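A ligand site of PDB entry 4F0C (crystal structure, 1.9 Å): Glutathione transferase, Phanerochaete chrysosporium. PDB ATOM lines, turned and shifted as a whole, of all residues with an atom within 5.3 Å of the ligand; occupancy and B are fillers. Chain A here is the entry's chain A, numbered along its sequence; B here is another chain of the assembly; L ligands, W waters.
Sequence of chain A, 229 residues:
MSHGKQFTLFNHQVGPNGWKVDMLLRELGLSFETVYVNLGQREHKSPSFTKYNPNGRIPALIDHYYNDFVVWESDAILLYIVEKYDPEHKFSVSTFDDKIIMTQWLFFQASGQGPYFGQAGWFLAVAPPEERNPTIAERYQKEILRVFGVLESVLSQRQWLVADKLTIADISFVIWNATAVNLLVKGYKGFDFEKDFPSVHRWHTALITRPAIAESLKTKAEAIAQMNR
A ring nitrogen (NE2) of His 44 sits at hydrogen-bond distance from an oxygen (O5) of the ligand (2.7 Å). The side-chain amino group (NZ) of Lys 20 lies within salt-bridge range of an oxygen (O1) of the ligand (3.9 Å). The side-chain hydroxyl (OG) of Ser 74 lies within hydrogen-bond range of an oxygen (O1) of the ligand. The backbone carbonyl oxygen of Ile 58 sits at hydrogen-bond distance from a nitrogen (N2) of the ligand (2.8 Å). O5 of the ligand is in salt-bridge range of NZ of Lys 45, at 3.9 Å. N1 of the ligand is in salt-bridge range of OE1 of Glu 73 (2.7 Å). An oxygen (O6) of the ligand lies within salt-bridge range of the guanidinium group (NE) of Arg 57 (3.1 Å). ND2 of Asn 17 sits at hydrogen-bond distance from O7 of the ligand. OG of Ser 111 of chain B sits at hydrogen-bond distance from N1 of the ligand (2.8 Å). O11 of the ligand is in salt-bridge range of NH2 of Arg 139 of chain B. The backbone NH of Ser 74 lies within hydrogen-bond range of an oxygen (O2) of the ligand (2.9 Å). N of Ile 58 sits at hydrogen-bond distance from O4 of the ligand.
The side-chain amide nitrogen of Gln 119 sits at hydrogen-bond distance from the backbone carbonyl oxygen of Pro 115, at 2.9 Å. The side-chain amino group (NZ) of Lys 20 sits at hydrogen-bond distance from the side-chain hydroxyl (OG) of Ser 74 (2.7 Å). The backbone NH of Gly 15 sits at hydrogen-bond distance from a ring nitrogen (ND1) of His 12 (3.1 Å). NH1 of Arg 57 lies within hydrogen-bond range of OH of Tyr 116 of chain B (3.4 Å). The side-chain amide oxygen of Gln 119 sits at hydrogen-bond distance from the guanidinium group of Arg 139 of chain B (2.8 Å). The side-chain hydroxyl (OG) of Ser 111 of chain B lies within hydrogen-bond range of the backbone carbonyl oxygen (O) of Phe 107 of chain B, at 2.7 Å. The side-chain amino group (NZ) of Lys 20 lies within salt-bridge range of the side-chain carboxylate (OD1) of Asp 75 (3.0 Å). The side-chain carboxylate of Glu 73 sits at hydrogen-bond distance from the side-chain hydroxyl of Ser 111 of chain B.
The backbone nitrogen (N) of Pro 16 lies close to a sulfur (S1) of the ligand (3.8 Å). An oxygen (O8) of the ligand sits close to the backbone nitrogen (N) of Pro 115, at 3.2 Å. Residues that only touch the ligand: Gly 15 (3.5 Å), Pro 59 (3.5 Å), Gly 114 (3.3 Å), Gly 118 (3.3 Å), Trp 122 (3.8 Å), Trp 176 (3.5 Å) and Tyr 116 of chain B (3.4 Å). Hydrophobic or aromatic side chains within 4 Å of the ligand: Pro 16, His 44, Ile 58, Pro 59, Pro 115, Trp 122 and Trp 176. 19 residues have an atom within 4 Å of the ligand: Gly 15, Pro 16, Asn 17, Lys 20, His 44, Lys 45, Arg 57, Ile 58, Pro 59, Glu 73, Ser 74, Gly 114, Pro 115, Gly 118, Trp 122, Trp 176, Ser 111 of chain B, Tyr 116 of chain B and Arg 139 of chain B. The nearest printed residue that does not touch the ligand is Leu 39 (4.1 Å).
Water W4 lies within hydrogen-bond range of O9 of the ligand, OH of Tyr 116 of chain B and NE2 of Gln 119. Water W12 lies within hydrogen-bond range of O2 of the ligand (2.7 Å), O of Pro 59 (2.9 Å) and N of Glu 73 (3.0 Å). Water W5 lies within hydrogen-bond range of OE2 of Glu 73 (2.7 Å), OG of Ser 111 of chain B (2.9 Å) and N1 of the ligand (3.0 Å). Water W7 bridges an oxygen (O10) of the ligand and the guanidinium group (NH1) of Arg 139 of chain B. Water W10 lies within hydrogen-bond range of OE1 of Glu 73 (2.9 Å), N of Asp 75 (3.0 Å), O1 of the ligand (3.1 Å) and OG of Ser 74 (3.5 Å). Water W9 lies within hydrogen-bond range of the side-chain amide oxygen of Asn 17 (2.7 Å), the side-chain amino group of Lys 20 (2.8 Å), an oxygen (O7) of the ligand (3.2 Å) and the indole nitrogen of Trp 176 (3.5 Å).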
ATOM      1  N   HIS A  12      10.264  17.531   6.324  1.00  0.00           N
ATOM      2  CA  HIS A  12      11.177  17.801   5.209  1.00  0.00           C
ATOM      3  C   HIS A  12      10.299  18.057   3.984  1.00  0.00           C
ATOM      4  O   HIS A  12       9.230  17.454   3.853  1.00  0.00           O
ATOM      5  CB  HIS A  12      12.102  16.596   4.945  1.00  0.00           C
ATOM      6  CG  HIS A  12      13.221  16.919   3.994  1.00  0.00           C
ATOM      7  ND1 HIS A  12      13.245  16.469   2.697  1.00  0.00           N
ATOM      8  CD2 HIS A  12      14.312  17.710   4.145  1.00  0.00           C
ATOM      9  CE1 HIS A  12      14.327  16.939   2.088  1.00  0.00           C
ATOM     10  NE2 HIS A  12      14.991  17.689   2.942  1.00  0.00           N
ATOM     11  N   GLY A  15      11.080  14.675   1.333  1.00  0.00           N
ATOM     12  CA  GLY A  15      10.851  13.337   1.878  1.00  0.00           C
ATOM     13  C   GLY A  15       9.389  13.120   2.244  1.00  0.00           C
ATOM     14  O   GLY A  15       8.730  14.028   2.763  1.00  0.00           O
ATOM     15  N   PRO A  16       8.852  11.920   1.979  1.00  0.00           N
ATOM     16  CA  PRO A  16       7.391  11.778   2.160  1.00  0.00           C
ATOM     17  C   PRO A  16       6.929  11.727   3.602  1.00  0.00           C
ATOM     18  O   PRO A  16       5.826  12.199   3.883  1.00  0.00           O
ATOM     19  CB  PRO A  16       7.104  10.415   1.460  1.00  0.00           C
ATOM     20  CG  PRO A  16       8.160  10.370   0.386  1.00  0.00           C
ATOM     21  CD  PRO A  16       9.401  10.876   1.099  1.00  0.00           C
ATOM     22  N   ASN A  17       7.722  11.152   4.513  1.00  0.00           N
ATOM     23  CA  ASN A  17       7.125  10.643   5.738  1.00  0.00           C
ATOM     24  C   ASN A  17       6.469  11.644   6.696  1.00  0.00           C
ATOM     25  O   ASN A  17       5.457  11.326   7.329  1.00  0.00           O
ATOM     26  CB  ASN A  17       8.149   9.766   6.475  1.00  0.00           C
ATOM     27  CG  ASN A  17       8.357   8.458   5.769  1.00  0.00           C
ATOM     28  OD1 ASN A  17       7.394   7.740   5.511  1.00  0.00           O
ATOM     29  ND2 ASN A  17       9.575   8.181   5.373  1.00  0.00           N
ATOM     30  N   LYS A  20       2.481  12.513   6.311  1.00  0.00           N
ATOM     31  CA  LYS A  20       1.411  11.751   6.951  1.00  0.00           C
ATOM     32  C   LYS A  20       0.891  12.520   8.160  1.00  0.00           C
ATOM     33  O   LYS A  20      -0.327  12.583   8.398  1.00  0.00           O
ATOM     34  CB  LYS A  20       1.906  10.403   7.498  1.00  0.00           C
ATOM     35  CG  LYS A  20       2.523   9.450   6.455  1.00  0.00           C
ATOM     36  CD  LYS A  20       3.086   8.250   7.259  1.00  0.00           C
ATOM     37  CE  LYS A  20       4.086   7.417   6.432  1.00  0.00           C
ATOM     38  NZ  LYS A  20       4.708   6.381   7.340  1.00  0.00           N
ATOM     39  N   LEU A  39      18.618  18.174   5.639  1.00  0.00           N
ATOM     40  CA  LEU A  39      19.354  16.915   5.591  1.00  0.00           C
ATOM     41  C   LEU A  39      20.737  17.064   4.900  1.00  0.00           C
ATOM     42  O   LEU A  39      21.636  16.245   5.127  1.00  0.00           O
ATOM     43  CB  LEU A  39      18.487  15.842   4.913  1.00  0.00           C
ATOM     44  CG  LEU A  39      17.023  15.780   5.394  1.00  0.00           C
ATOM     45  CD1 LEU A  39      16.197  14.753   4.608  1.00  0.00           C
ATOM     46  CD2 LEU A  39      16.900  15.515   6.909  1.00  0.00           C
ATOM     47  N   HIS A  44      19.887  16.780  10.701  1.00  0.00           N
ATOM     48  CA  HIS A  44      19.117  15.690  11.317  1.00  0.00           C
ATOM     49  C   HIS A  44      19.999  14.706  12.105  1.00  0.00           C
ATOM     50  O   HIS A  44      19.495  13.919  12.901  1.00  0.00           O
ATOM     51  CB  HIS A  44      18.321  14.948  10.237  1.00  0.00           C
ATOM     52  CG  HIS A  44      19.166  14.364   9.160  1.00  0.00           C
ATOM     53  ND1 HIS A  44      20.044  15.127   8.403  1.00  0.00           N
ATOM     54  CD2 HIS A  44      19.285  13.092   8.693  1.00  0.00           C
ATOM     55  CE1 HIS A  44      20.660  14.341   7.525  1.00  0.00           C
ATOM     56  NE2 HIS A  44      20.210  13.107   7.683  1.00  0.00           N
ATOM     57  N   LYS A  45      21.323  14.770  11.887  1.00  0.00           N
ATOM     58  CA  LYS A  45      22.268  13.902  12.589  1.00  0.00           C
ATOM     59  C   LYS A  45      23.047  14.681  13.661  1.00  0.00           C
ATOM     60  O   LYS A  45      23.944  14.137  14.309  1.00  0.00           O
ATOM     61  CB  LYS A  45      23.267  13.260  11.597  1.00  0.00           C
ATOM     62  CG  LYS A  45      22.633  12.417  10.466  1.00  0.00           C
ATOM     63  CD  LYS A  45      21.538  11.469  10.975  1.00  0.00           C
ATOM     64  CE  LYS A  45      21.247  10.349   9.955  1.00  0.00           C
ATOM     65  NZ  LYS A  45      20.125   9.445  10.385  1.00  0.00           N
ATOM     66  N   GLY A  56      17.733   9.967  14.292  1.00  0.00           N
ATOM     67  CA  GLY A  56      18.187  11.062  13.414  1.00  0.00           C
ATOM     68  C   GLY A  56      17.491  11.071  12.047  1.00  0.00           C
ATOM     69  O   GLY A  56      18.098  11.368  11.009  1.00  0.00           O
ATOM     70  N   ARG A  57      16.209  10.760  12.053  1.00  0.00           N
ATOM     71  CA  ARG A  57      15.376  10.824  10.839  1.00  0.00           C
ATOM     72  C   ARG A  57      14.100  11.590  11.157  1.00  0.00           C
ATOM     73  O   ARG A  57      13.649  11.607  12.298  1.00  0.00           O
ATOM     74  CB  ARG A  57      15.053   9.420  10.301  1.00  0.00           C
ATOM     75  CG  ARG A  57      16.304   8.630   9.887  1.00  0.00           C
ATOM     76  CD  ARG A  57      15.888   7.274   9.239  1.00  0.00           C
ATOM     77  NE  ARG A  57      15.905   7.310   7.767  1.00  0.00           N
ATOM     78  CZ  ARG A  57      15.471   6.320   6.979  1.00  0.00           C
ATOM     79  NH1 ARG A  57      14.926   5.234   7.508  1.00  0.00           N
ATOM     80  NH2 ARG A  57      15.551   6.436   5.657  1.00  0.00           N
ATOM     81  N   ILE A  58      13.541  12.267  10.154  1.00  0.00           N
ATOM     82  CA  ILE A  58      12.274  12.962  10.348  1.00  0.00           C
ATOM     83  C   ILE A  58      11.124  12.032   9.906  1.00  0.00           C
ATOM     84  O   ILE A  58      11.311  11.168   9.049  1.00  0.00           O
ATOM     85  CB  ILE A  58      12.256  14.337   9.592  1.00  0.00           C
ATOM     86  CG1 ILE A  58      12.190  14.131   8.095  1.00  0.00           C
ATOM     87  CG2 ILE A  58      13.441  15.219  10.006  1.00  0.00           C
ATOM     88  CD1 ILE A  58      10.786  14.181   7.571  1.00  0.00           C
ATOM     89  N   PRO A  59       9.908  12.232  10.455  1.00  0.00           N
ATOM     90  CA  PRO A  59       9.507  13.311  11.370  1.00  0.00           C
ATOM     91  C   PRO A  59       9.748  13.026  12.865  1.00  0.00           C
ATOM     92  O   PRO A  59      10.007  11.891  13.299  1.00  0.00           O
ATOM     93  CB  PRO A  59       8.006  13.407  11.135  1.00  0.00           C
ATOM     94  CG  PRO A  59       7.619  11.956  10.887  1.00  0.00           C
ATOM     95  CD  PRO A  59       8.743  11.459   9.979  1.00  0.00           C
ATOM     96  N   GLU A  73       9.050   8.346  14.688  1.00  0.00           N
ATOM     97  CA  GLU A  73       8.388   7.359  13.817  1.00  0.00           C
ATOM     98  C   GLU A  73       7.032   7.929  13.396  1.00  0.00           C
ATOM     99  O   GLU A  73       6.112   8.049  14.219  1.00  0.00           O
ATOM    100  CB  GLU A  73       8.225   5.962  14.448  1.00  0.00           C
ATOM    101  CG  GLU A  73       9.537   5.139  14.483  1.00  0.00           C
ATOM    102  CD  GLU A  73      10.128   4.909  13.088  1.00  0.00           C
ATOM    103  OE1 GLU A  73       9.379   4.591  12.137  1.00  0.00           O
ATOM    104  OE2 GLU A  73      11.366   5.075  12.929  1.00  0.00           O
ATOM    105  N   SER A  74       6.933   8.300  12.136  1.00  0.00           N
ATOM    106  CA  SER A  74       5.686   8.869  11.599  1.00  0.00           C
ATOM    107  C   SER A  74       4.416   8.113  12.042  1.00  0.00           C
ATOM    108  O   SER A  74       3.443   8.762  12.440  1.00  0.00           O
ATOM    109  CB  SER A  74       5.740   8.978  10.051  1.00  0.00           C
ATOM    110  OG  SER A  74       5.914   7.712   9.385  1.00  0.00           O
ATOM    111  N   ASP A  75       4.414   6.778  12.002  1.00  0.00           N
ATOM    112  CA  ASP A  75       3.158   6.086  12.301  1.00  0.00           C
ATOM    113  C   ASP A  75       2.876   6.044  13.796  1.00  0.00           C
ATOM    114  O   ASP A  75       1.707   5.973  14.223  1.00  0.00           O
ATOM    115  CB  ASP A  75       3.127   4.653  11.717  1.00  0.00           C
ATOM    116  CG  ASP A  75       2.965   4.629  10.211  1.00  0.00           C
ATOM    117  OD1 ASP A  75       2.830   5.719   9.561  1.00  0.00           O
ATOM    118  OD2 ASP A  75       2.936   3.517   9.664  1.00  0.00           O
ATOM    119  N   ALA A 110       4.231   0.803   7.553  1.00  0.00           N
ATOM    120  CA  ALA A 110       5.569   1.208   8.010  1.00  0.00           C
ATOM    121  C   ALA A 110       6.708   0.282   7.567  1.00  0.00           C
ATOM    122  O   ALA A 110       7.847   0.738   7.377  1.00  0.00           O
ATOM    123  CB  ALA A 110       5.586   1.351   9.542  1.00  0.00           C
ATOM    124  N   GLY A 114       6.594   2.126   3.086  1.00  0.00           N
ATOM    125  CA  GLY A 114       7.703   3.095   3.192  1.00  0.00           C
ATOM    126  C   GLY A 114       9.095   2.568   2.796  1.00  0.00           C
ATOM    127  O   GLY A 114       9.731   3.131   1.925  1.00  0.00           O
ATOM    128  N   PRO A 115       9.543   1.472   3.429  1.00  0.00           N
ATOM    129  CA  PRO A 115      10.941   1.092   3.220  1.00  0.00           C
ATOM    130  C   PRO A 115      11.196   0.615   1.793  1.00  0.00           C
ATOM    131  O   PRO A 115      12.207   1.021   1.214  1.00  0.00           O
ATOM    132  CB  PRO A 115      11.154  -0.054   4.234  1.00  0.00           C
ATOM    133  CG  PRO A 115      10.172   0.271   5.369  1.00  0.00           C
ATOM    134  CD  PRO A 115       8.932   0.702   4.534  1.00  0.00           C
ATOM    135  N   GLY A 118      10.693   3.466  -0.677  1.00  0.00           N
ATOM    136  CA  GLY A 118      11.869   4.281  -0.481  1.00  0.00           C
ATOM    137  C   GLY A 118      13.116   3.778  -1.200  1.00  0.00           C
ATOM    138  O   GLY A 118      13.929   4.587  -1.649  1.00  0.00           O
ATOM    139  N   GLN A 119      13.288   2.458  -1.313  1.00  0.00           N
ATOM    140  CA  GLN A 119      14.464   1.941  -2.022  1.00  0.00           C
ATOM    141  C   GLN A 119      14.290   2.223  -3.509  1.00  0.00           C
ATOM    142  O   GLN A 119      15.261   2.583  -4.169  1.00  0.00           O
ATOM    143  CB  GLN A 119      14.694   0.448  -1.795  1.00  0.00           C
ATOM    144  CG  GLN A 119      14.880   0.053  -0.348  1.00  0.00           C
ATOM    145  CD  GLN A 119      15.683   1.064   0.404  1.00  0.00           C
ATOM    146  OE1 GLN A 119      16.881   1.233   0.167  1.00  0.00           O
ATOM    147  NE2 GLN A 119      15.025   1.765   1.339  1.00  0.00           N
ATOM    148  N   TRP A 122      15.245   5.830  -3.838  1.00  0.00           N
ATOM    149  CA  TRP A 122      16.694   5.960  -3.751  1.00  0.00           C
ATOM    150  C   TRP A 122      17.337   5.634  -5.095  1.00  0.00           C
ATOM    151  O   TRP A 122      18.002   6.496  -5.691  1.00  0.00           O
ATOM    152  CB  TRP A 122      17.286   5.035  -2.674  1.00  0.00           C
ATOM    153  CG  TRP A 122      18.785   5.167  -2.531  1.00  0.00           C
ATOM    154  CD1 TRP A 122      19.728   4.277  -2.950  1.00  0.00           C
ATOM    155  CD2 TRP A 122      19.493   6.261  -1.936  1.00  0.00           C
ATOM    156  NE1 TRP A 122      20.998   4.757  -2.640  1.00  0.00           N
ATOM    157  CE2 TRP A 122      20.873   5.973  -2.020  1.00  0.00           C
ATOM    158  CE3 TRP A 122      19.088   7.464  -1.338  1.00  0.00           C
ATOM    159  CZ2 TRP A 122      21.851   6.835  -1.517  1.00  0.00           C
ATOM    160  CZ3 TRP A 122      20.068   8.323  -0.844  1.00  0.00           C
ATOM    161  CH2 TRP A 122      21.421   7.998  -0.931  1.00  0.00           C
ATOM    162  N   VAL A 126      16.490   9.835  -5.958  1.00  0.00           N
ATOM    163  CA  VAL A 126      16.861  10.592  -4.771  1.00  0.00           C
ATOM    164  C   VAL A 126      18.312  10.414  -4.372  1.00  0.00           C
ATOM    165  O   VAL A 126      18.907  11.296  -3.743  1.00  0.00           O
ATOM    166  CB  VAL A 126      15.889  10.254  -3.600  1.00  0.00           C
ATOM    167  CG1 VAL A 126      16.649  10.000  -2.295  1.00  0.00           C
ATOM    168  CG2 VAL A 126      14.841  11.359  -3.449  1.00  0.00           C
ATOM    169  N   TRP A 176       3.194   8.049   0.244  1.00  0.00           N
ATOM    170  CA  TRP A 176       4.021   7.158  -0.570  1.00  0.00           C
ATOM    171  C   TRP A 176       3.290   6.658  -1.820  1.00  0.00           C
ATOM    172  O   TRP A 176       3.921   6.432  -2.864  1.00  0.00           O
ATOM    173  CB  TRP A 176       4.561   5.983   0.228  1.00  0.00           C
ATOM    174  CG  TRP A 176       5.795   6.300   1.049  1.00  0.00           C
ATOM    175  CD1 TRP A 176       5.877   6.423   2.417  1.00  0.00           C
ATOM    176  CD2 TRP A 176       7.126   6.533   0.543  1.00  0.00           C
ATOM    177  NE1 TRP A 176       7.164   6.717   2.772  1.00  0.00           N
ATOM    178  CE2 TRP A 176       7.954   6.776   1.655  1.00  0.00           C
ATOM    179  CE3 TRP A 176       7.691   6.530  -0.739  1.00  0.00           C
ATOM    180  CZ2 TRP A 176       9.317   7.049   1.530  1.00  0.00           C
ATOM    181  CZ3 TRP A 176       9.056   6.799  -0.874  1.00  0.00           C
ATOM    182  CH2 TRP A 176       9.849   7.045   0.250  1.00  0.00           C
ATOM    183  N   PHE B 107       7.792   0.458  16.083  1.00  0.00           N
ATOM    184  CA  PHE B 107       7.780   0.991  14.713  1.00  0.00           C
ATOM    185  C   PHE B 107       9.189   1.177  14.191  1.00  0.00           C
ATOM    186  O   PHE B 107       9.446   0.967  13.001  1.00  0.00           O
ATOM    187  CB  PHE B 107       6.972   2.285  14.584  1.00  0.00           C
ATOM    188  CG  PHE B 107       5.489   2.020  14.310  1.00  0.00           C
ATOM    189  CD1 PHE B 107       5.051   1.704  13.007  1.00  0.00           C
ATOM    190  CD2 PHE B 107       4.561   2.007  15.351  1.00  0.00           C
ATOM    191  CE1 PHE B 107       3.690   1.411  12.764  1.00  0.00           C
ATOM    192  CE2 PHE B 107       3.202   1.730  15.114  1.00  0.00           C
ATOM    193  CZ  PHE B 107       2.773   1.417  13.834  1.00  0.00           C
ATOM    194  N   SER B 111      10.297  -0.786  10.789  1.00  0.00           N
ATOM    195  CA  SER B 111      10.538   0.010   9.578  1.00  0.00           C
ATOM    196  C   SER B 111      12.039   0.237   9.362  1.00  0.00           C
ATOM    197  O   SER B 111      12.496   0.465   8.247  1.00  0.00           O
ATOM    198  CB  SER B 111       9.796   1.369   9.661  1.00  0.00           C
ATOM    199  OG  SER B 111      10.296   2.175  10.740  1.00  0.00           O
ATOM    200  N   GLY B 112      12.805   0.194  10.440  1.00  0.00           N
ATOM    201  CA  GLY B 112      14.203   0.621  10.372  1.00  0.00           C
ATOM    202  C   GLY B 112      15.159  -0.557  10.603  1.00  0.00           C
ATOM    203  O   GLY B 112      16.297  -0.491  10.170  1.00  0.00           O
ATOM    204  N   TYR B 116      15.715  -3.129   6.340  1.00  0.00           N
ATOM    205  CA  TYR B 116      17.073  -2.845   5.887  1.00  0.00           C
ATOM    206  C   TYR B 116      17.980  -4.041   6.146  1.00  0.00           C
ATOM    207  O   TYR B 116      18.806  -4.383   5.321  1.00  0.00           O
ATOM    208  CB  TYR B 116      17.626  -1.605   6.616  1.00  0.00           C
ATOM    209  CG  TYR B 116      16.934  -0.341   6.142  1.00  0.00           C
ATOM    210  CD1 TYR B 116      17.369   0.337   5.006  1.00  0.00           C
ATOM    211  CD2 TYR B 116      15.806   0.150   6.807  1.00  0.00           C
ATOM    212  CE1 TYR B 116      16.713   1.518   4.552  1.00  0.00           C
ATOM    213  CE2 TYR B 116      15.137   1.314   6.356  1.00  0.00           C
ATOM    214  CZ  TYR B 116      15.597   1.984   5.230  1.00  0.00           C
ATOM    215  OH  TYR B 116      14.925   3.128   4.787  1.00  0.00           O
ATOM    216  N   ARG B 139      25.696  -1.323   1.051  1.00  0.00           N
ATOM    217  CA  ARG B 139      24.818  -0.238   1.443  1.00  0.00           C
ATOM    218  C   ARG B 139      23.988  -0.629   2.672  1.00  0.00           C
ATOM    219  O   ARG B 139      23.813   0.174   3.612  1.00  0.00           O
ATOM    220  CB  ARG B 139      23.884   0.159   0.257  1.00  0.00           C
ATOM    221  CG  ARG B 139      22.522   0.783   0.676  1.00  0.00           C
ATOM    222  CD  ARG B 139      21.729   1.311  -0.559  1.00  0.00           C
ATOM    223  NE  ARG B 139      20.378   1.760  -0.211  1.00  0.00           N
ATOM    224  CZ  ARG B 139      20.073   2.947   0.320  1.00  0.00           C
ATOM    225  NH1 ARG B 139      21.009   3.841   0.566  1.00  0.00           N
ATOM    226  NH2 ARG B 139      18.810   3.236   0.633  1.00  0.00           N
HETATM  227  N1  LIG L   1      10.204   4.674   9.535  1.00  0.00           N
HETATM  228  C1  LIG L   1      10.506   6.149   9.574  1.00  0.00           C
HETATM  229  C2  LIG L   1       9.179   7.000   9.723  1.00  0.00           C
HETATM  230  O1  LIG L   1       8.117   6.583   9.174  1.00  0.00           O
HETATM  231  O2  LIG L   1       9.244   8.030  10.455  1.00  0.00           O
HETATM  232  C3  LIG L   1      11.264   6.632   8.278  1.00  0.00           C
HETATM  233  C4  LIG L   1      11.570   8.144   8.336  1.00  0.00           C
HETATM  234  C5  LIG L   1      12.430   8.509   7.170  1.00  0.00           C
HETATM  235  O3  LIG L   1      12.799   7.730   6.303  1.00  0.00           O
HETATM  236  N2  LIG L   1      12.796   9.833   7.142  1.00  0.00           N
HETATM  237  C6  LIG L   1      13.674  10.381   6.083  1.00  0.00           C
HETATM  238  C7  LIG L   1      14.926  10.950   6.697  1.00  0.00           C
HETATM  239  O4  LIG L   1      14.859  11.628   7.725  1.00  0.00           O
HETATM  240  C8  LIG L   1      12.998  11.575   5.364  1.00  0.00           C
HETATM  241  S1  LIG L   1      11.648  10.971   4.318  1.00  0.00           S
HETATM  242  N3  LIG L   1      16.082  10.754   6.019  1.00  0.00           N
HETATM  243  C9  LIG L   1      17.300  11.314   6.528  1.00  0.00           C
HETATM  244  C10 LIG L   1      18.424  10.291   6.496  1.00  0.00           C
HETATM  245  O5  LIG L   1      19.593  10.697   6.677  1.00  0.00           O
HETATM  246  O6  LIG L   1      18.061   9.100   6.360  1.00  0.00           O
HETATM  247  N4  LIG L   1      12.402   5.943   4.117  1.00  0.00           N
HETATM  248  C11 LIG L   1      11.927   4.555   4.231  1.00  0.00           C
HETATM  249  C12 LIG L   1      10.567   4.564   4.975  1.00  0.00           C
HETATM  250  O7  LIG L   1       9.804   5.553   4.825  1.00  0.00           O
HETATM  251  O8  LIG L   1      10.315   3.558   5.669  1.00  0.00           O
HETATM  252  C13 LIG L   1      13.118   6.347   3.008  1.00  0.00           C
HETATM  253  O9  LIG L   1      13.395   5.611   2.067  1.00  0.00           O
HETATM  254  C14 LIG L   1      13.546   7.805   2.953  1.00  0.00           C
HETATM  255  N5  LIG L   1      14.797   7.944   2.144  1.00  0.00           N
HETATM  256  C15 LIG L   1      12.405   8.610   2.315  1.00  0.00           C
HETATM  257  S2  LIG L   1      12.690  10.404   2.520  1.00  0.00           S
HETATM  258  C16 LIG L   1      18.666   7.376   3.497  1.00  0.00           C
HETATM  259  C17 LIG L   1      19.048   6.156   2.556  1.00  0.00           C
HETATM  260  O10 LIG L   1      20.236   5.796   2.518  1.00  0.00           O
HETATM  261  O11 LIG L   1      18.110   5.627   1.919  1.00  0.00           O
HETATM  262  N6  LIG L   1      19.699   7.574   4.513  1.00  0.00           N
HETATM  263  C18 LIG L   1      18.478   8.621   2.583  1.00  0.00           C
HETATM  264  C19 LIG L   1      17.152   8.591   1.790  1.00  0.00           C
HETATM  265  C20 LIG L   1      15.957   8.499   2.739  1.00  0.00           C
HETATM  266  O12 LIG L   1      15.935   8.895   3.904  1.00  0.00           O
HETATM  267  O   HOH W   1      12.021   3.300   7.740  1.00  0.00           O
HETATM  268  O   HOH W   2       8.346   3.474   7.380  1.00  0.00           O
HETATM  269  O   HOH W   3      19.731   7.705   8.335  1.00  0.00           O
HETATM  270  O   HOH W   4      15.725   4.497   2.481  1.00  0.00           O
HETATM  271  O   HOH W   5      12.697   3.767  10.993  1.00  0.00           O
HETATM  272  O   HOH W   6      14.653   7.209  -0.578  1.00  0.00           O
HETATM  273  O   HOH W   7      20.537   3.128   3.944  1.00  0.00           O
HETATM  274  O   HOH W   8      21.228   6.126   6.152  1.00  0.00           O
HETATM  275  O   HOH W   9       6.765   5.181   5.868  1.00  0.00           O
HETATM  276  O   HOH W  10       6.626   4.875  11.284  1.00  0.00           O
HETATM  277  O   HOH W  11      22.129  10.239   6.060  1.00  0.00           O
HETATM  278  O   HOH W  12      10.761   9.283  12.368  1.00  0.00           O
